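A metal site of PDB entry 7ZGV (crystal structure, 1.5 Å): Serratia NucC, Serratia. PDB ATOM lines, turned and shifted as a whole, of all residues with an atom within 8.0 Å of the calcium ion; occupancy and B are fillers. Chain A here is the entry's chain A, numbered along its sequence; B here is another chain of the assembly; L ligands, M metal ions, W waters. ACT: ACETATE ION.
Three residues have an atom within 4 Å of the calcium ion: Ser 80, Val 250 and Asp 253.
The calcium ion is bound by O of Val 250 (2.3 Å), water W2 (2.3 Å), O of Ser 80 (2.3 Å), OD1 of Asp 253 (2.4 Å), water W1 (2.4 Å), OXT of the ligand (2.4 Å) and O of the ligand (2.5 Å).
The calcium ion has seven donor atoms within binding distance.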
ATOM      1  N   ASP A  79       4.923  14.850  -9.913  1.00  0.00           N
ATOM      2  CA  ASP A  79       6.119  14.122  -9.512  1.00  0.00           C
ATOM      3  C   ASP A  79       7.293  14.458 -10.434  1.00  0.00           C
ATOM      4  O   ASP A  79       7.131  15.170 -11.435  1.00  0.00           O
ATOM      5  CB  ASP A  79       5.861  12.607  -9.378  1.00  0.00           C
ATOM      6  CG  ASP A  79       5.683  11.895 -10.704  1.00  0.00           C
ATOM      7  OD1 ASP A  79       6.011  12.417 -11.810  1.00  0.00           O
ATOM      8  OD2 ASP A  79       5.264  10.715 -10.642  1.00  0.00           O
ATOM      9  N   SER A  80       8.471  13.887 -10.127  1.00  0.00           N
ATOM     10  CA  SER A  80       9.709  14.133 -10.866  1.00  0.00           C
ATOM     11  C   SER A  80       9.764  13.440 -12.209  1.00  0.00           C
ATOM     12  O   SER A  80      10.764  13.589 -12.921  1.00  0.00           O
ATOM     13  CB  SER A  80      10.908  13.677 -10.032  1.00  0.00           C
ATOM     14  OG  SER A  80      10.795  12.317  -9.667  1.00  0.00           O
ATOM     15  N   GLU A  81       8.748  12.634 -12.539  1.00  0.00           N
ATOM     16  CA  GLU A  81       8.574  12.025 -13.838  1.00  0.00           C
ATOM     17  C   GLU A  81       7.635  12.846 -14.715  1.00  0.00           C
ATOM     18  O   GLU A  81       7.294  12.423 -15.820  1.00  0.00           O
ATOM     19  CB  GLU A  81       8.023  10.613 -13.663  1.00  0.00           C
ATOM     20  CG  GLU A  81       8.968   9.667 -12.923  1.00  0.00           C
ATOM     21  CD  GLU A  81      10.127   9.207 -13.773  1.00  0.00           C
ATOM     22  OE1 GLU A  81       9.895   8.973 -14.960  1.00  0.00           O
ATOM     23  OE2 GLU A  81      11.252   9.094 -13.250  1.00  0.00           O
ATOM     24  N   GLY A  82       7.213  14.006 -14.228  1.00  0.00           N
ATOM     25  CA  GLY A  82       6.304  14.833 -15.011  1.00  0.00           C
ATOM     26  C   GLY A  82       4.844  14.417 -14.938  1.00  0.00           C
ATOM     27  O   GLY A  82       4.015  14.995 -15.646  1.00  0.00           O
ATOM     28  N   TYR A 144       5.368   9.119  -8.235  1.00  0.00           N
ATOM     29  CA  TYR A 144       6.661   8.688  -7.746  1.00  0.00           C
ATOM     30  C   TYR A 144       7.196   9.645  -6.689  1.00  0.00           C
ATOM     31  O   TYR A 144       7.112  10.865  -6.848  1.00  0.00           O
ATOM     32  CB  TYR A 144       7.638   8.615  -8.927  1.00  0.00           C
ATOM     33  CG  TYR A 144       9.013   8.122  -8.551  1.00  0.00           C
ATOM     34  CD1 TYR A 144       9.218   6.854  -8.072  1.00  0.00           C
ATOM     35  CD2 TYR A 144      10.118   8.944  -8.715  1.00  0.00           C
ATOM     36  CE1 TYR A 144      10.490   6.402  -7.734  1.00  0.00           C
ATOM     37  CE2 TYR A 144      11.395   8.520  -8.381  1.00  0.00           C
ATOM     38  CZ  TYR A 144      11.570   7.256  -7.900  1.00  0.00           C
ATOM     39  OH  TYR A 144      12.843   6.869  -7.563  1.00  0.00           O
ATOM     40  N   TRP A 248      16.395  16.791  -4.785  1.00  0.00           N
ATOM     41  CA  TRP A 248      16.293  17.964  -5.641  1.00  0.00           C
ATOM     42  C   TRP A 248      16.774  17.677  -7.056  1.00  0.00           C
ATOM     43  O   TRP A 248      16.365  18.378  -7.994  1.00  0.00           O
ATOM     44  CB  TRP A 248      17.105  19.109  -5.016  1.00  0.00           C
ATOM     45  CG  TRP A 248      18.507  18.721  -4.754  1.00  0.00           C
ATOM     46  CD1 TRP A 248      19.017  18.171  -3.609  1.00  0.00           C
ATOM     47  CD2 TRP A 248      19.600  18.787  -5.689  1.00  0.00           C
ATOM     48  NE1 TRP A 248      20.355  17.927  -3.762  1.00  0.00           N
ATOM     49  CE2 TRP A 248      20.740  18.284  -5.035  1.00  0.00           C
ATOM     50  CE3 TRP A 248      19.726  19.238  -7.004  1.00  0.00           C
ATOM     51  CZ2 TRP A 248      21.974  18.213  -5.650  1.00  0.00           C
ATOM     52  CZ3 TRP A 248      20.936  19.164  -7.616  1.00  0.00           C
ATOM     53  CH2 TRP A 248      22.062  18.658  -6.944  1.00  0.00           C
ATOM     54  N   ARG A 249      17.608  16.664  -7.260  1.00  0.00           N
ATOM     55  CA  ARG A 249      18.153  16.406  -8.586  1.00  0.00           C
ATOM     56  C   ARG A 249      17.077  15.975  -9.577  1.00  0.00           C
ATOM     57  O   ARG A 249      17.208  16.214 -10.783  1.00  0.00           O
ATOM     58  CB  ARG A 249      19.173  15.283  -8.482  1.00  0.00           C
ATOM     59  CG  ARG A 249      20.324  15.592  -7.512  1.00  0.00           C
ATOM     60  CD  ARG A 249      21.134  14.341  -7.113  1.00  0.00           C
ATOM     61  NE  ARG A 249      22.015  14.631  -5.989  1.00  0.00           N
ATOM     62  CZ  ARG A 249      21.643  14.647  -4.709  1.00  0.00           C
ATOM     63  NH1 ARG A 249      20.409  14.331  -4.328  1.00  0.00           N
ATOM     64  NH2 ARG A 249      22.524  15.030  -3.780  1.00  0.00           N
ATOM     65  N   VAL A 250      16.020  15.302  -9.116  1.00  0.00           N
ATOM     66  CA  VAL A 250      15.138  14.629 -10.061  1.00  0.00           C
ATOM     67  C   VAL A 250      14.113  15.566 -10.676  1.00  0.00           C
ATOM     68  O   VAL A 250      13.487  15.205 -11.689  1.00  0.00           O
ATOM     69  CB  VAL A 250      14.380  13.439  -9.424  1.00  0.00           C
ATOM     70  CG1 VAL A 250      15.356  12.355  -9.033  1.00  0.00           C
ATOM     71  CG2 VAL A 250      13.569  13.904  -8.235  1.00  0.00           C
ATOM     72  N   TYR A 251      13.934  16.759 -10.120  1.00  0.00           N
ATOM     73  CA  TYR A 251      13.052  17.739 -10.719  1.00  0.00           C
ATOM     74  C   TYR A 251      13.739  18.582 -11.798  1.00  0.00           C
ATOM     75  O   TYR A 251      13.066  19.402 -12.434  1.00  0.00           O
ATOM     76  CB  TYR A 251      12.420  18.603  -9.634  1.00  0.00           C
ATOM     77  CG  TYR A 251      11.284  17.867  -8.954  1.00  0.00           C
ATOM     78  CD1 TYR A 251      10.002  17.928  -9.453  1.00  0.00           C
ATOM     79  CD2 TYR A 251      11.510  17.089  -7.806  1.00  0.00           C
ATOM     80  CE1 TYR A 251       8.951  17.232  -8.859  1.00  0.00           C
ATOM     81  CE2 TYR A 251      10.441  16.383  -7.205  1.00  0.00           C
ATOM     82  CZ  TYR A 251       9.188  16.484  -7.755  1.00  0.00           C
ATOM     83  OH  TYR A 251       8.139  15.807  -7.184  1.00  0.00           O
ATOM     84  N   ILE A 252      15.036  18.403 -12.005  1.00  0.00           N
ATOM     85  CA  ILE A 252      15.756  19.144 -13.037  1.00  0.00           C
ATOM     86  C   ILE A 252      16.552  18.234 -13.979  1.00  0.00           C
ATOM     87  O   ILE A 252      17.241  18.738 -14.865  1.00  0.00           O
ATOM     88  CB  ILE A 252      16.655  20.250 -12.442  1.00  0.00           C
ATOM     89  CG1 ILE A 252      17.616  19.629 -11.421  1.00  0.00           C
ATOM     90  CG2 ILE A 252      15.806  21.364 -11.814  1.00  0.00           C
ATOM     91  CD1 ILE A 252      18.747  20.603 -10.967  1.00  0.00           C
ATOM     92  N   ASP A 253      16.465  16.919 -13.814  1.00  0.00           N
ATOM     93  CA  ASP A 253      17.335  16.019 -14.565  1.00  0.00           C
ATOM     94  C   ASP A 253      16.971  15.888 -16.043  1.00  0.00           C
ATOM     95  O   ASP A 253      17.835  15.496 -16.836  1.00  0.00           O
ATOM     96  CB  ASP A 253      17.452  14.657 -13.896  1.00  0.00           C
ATOM     97  CG  ASP A 253      16.097  13.955 -13.723  1.00  0.00           C
ATOM     98  OD1 ASP A 253      15.048  14.490 -14.163  1.00  0.00           O
ATOM     99  OD2 ASP A 253      16.123  12.842 -13.143  1.00  0.00           O
ATOM    100  N   SER A 254      15.745  16.217 -16.452  1.00  0.00           N
ATOM    101  CA  SER A 254      15.378  16.139 -17.854  1.00  0.00           C
ATOM    102  C   SER A 254      15.492  17.480 -18.576  1.00  0.00           C
ATOM    103  O   SER A 254      15.161  17.550 -19.758  1.00  0.00           O
ATOM    104  CB  SER A 254      13.949  15.621 -18.008  1.00  0.00           C
ATOM    105  OG  SER A 254      13.037  16.654 -17.672  1.00  0.00           O
ATOM    106  N   LEU A 255      15.959  18.527 -17.893  1.00  0.00           N
ATOM    107  CA  LEU A 255      16.028  19.862 -18.479  1.00  0.00           C
ATOM    108  C   LEU A 255      17.385  20.155 -19.083  1.00  0.00           C
ATOM    109  O   LEU A 255      18.428  19.698 -18.593  1.00  0.00           O
ATOM    110  CB  LEU A 255      15.709  20.900 -17.390  1.00  0.00           C
ATOM    111  CG  LEU A 255      14.372  20.674 -16.684  1.00  0.00           C
ATOM    112  CD1 LEU A 255      14.189  21.694 -15.561  1.00  0.00           C
ATOM    113  CD2 LEU A 255      13.220  20.736 -17.694  1.00  0.00           C
ATOM    114  N   ARG B  20       5.367  18.323 -16.934  1.00  0.00           N
ATOM    115  CA  ARG B  20       6.732  18.780 -17.159  1.00  0.00           C
ATOM    116  C   ARG B  20       6.723  20.173 -17.780  1.00  0.00           C
ATOM    117  O   ARG B  20       7.492  21.052 -17.400  1.00  0.00           O
ATOM    118  CB  ARG B  20       7.477  17.775 -18.049  1.00  0.00           C
ATOM    119  CG  ARG B  20       8.895  18.170 -18.365  1.00  0.00           C
ATOM    120  CD  ARG B  20       9.598  17.132 -19.230  1.00  0.00           C
ATOM    121  NE  ARG B  20      10.974  17.478 -19.530  1.00  0.00           N
ATOM    122  CZ  ARG B  20      11.332  18.235 -20.548  1.00  0.00           C
ATOM    123  NH1 ARG B  20      10.434  18.721 -21.400  1.00  0.00           N
ATOM    124  NH2 ARG B  20      12.617  18.506 -20.737  1.00  0.00           N
ATOM    125  N   LEU B  23       5.784  22.803 -15.212  1.00  0.00           N
ATOM    126  CA  LEU B  23       6.919  23.089 -14.338  1.00  0.00           C
ATOM    127  C   LEU B  23       7.906  24.030 -15.012  1.00  0.00           C
ATOM    128  O   LEU B  23       8.327  25.044 -14.433  1.00  0.00           O
ATOM    129  CB  LEU B  23       7.581  21.777 -13.922  1.00  0.00           C
ATOM    130  CG  LEU B  23       8.789  21.926 -13.003  1.00  0.00           C
ATOM    131  CD1 LEU B  23       8.470  22.532 -11.664  1.00  0.00           C
ATOM    132  CD2 LEU B  23       9.502  20.603 -12.813  1.00  0.00           C
HETATM  133  C   ACT L   1      12.018  17.049 -14.524  1.00  0.00           C
HETATM  134  O   ACT L   1      13.094  16.677 -15.023  1.00  0.00           O
HETATM  135  OXT ACT L   1      11.396  16.512 -13.580  1.00  0.00           O
HETATM  136  CH3 ACT L   1      11.405  18.339 -15.123  1.00  0.00           C
HETATM  137 CA    CA M   1      12.731  14.515 -13.757  1.00  0.00          CA
HETATM  138  O   HOH W   1      13.449  12.297 -13.252  1.00  0.00           O
HETATM  139  O   HOH W   2      12.004  13.776 -15.841  1.00  0.00           O
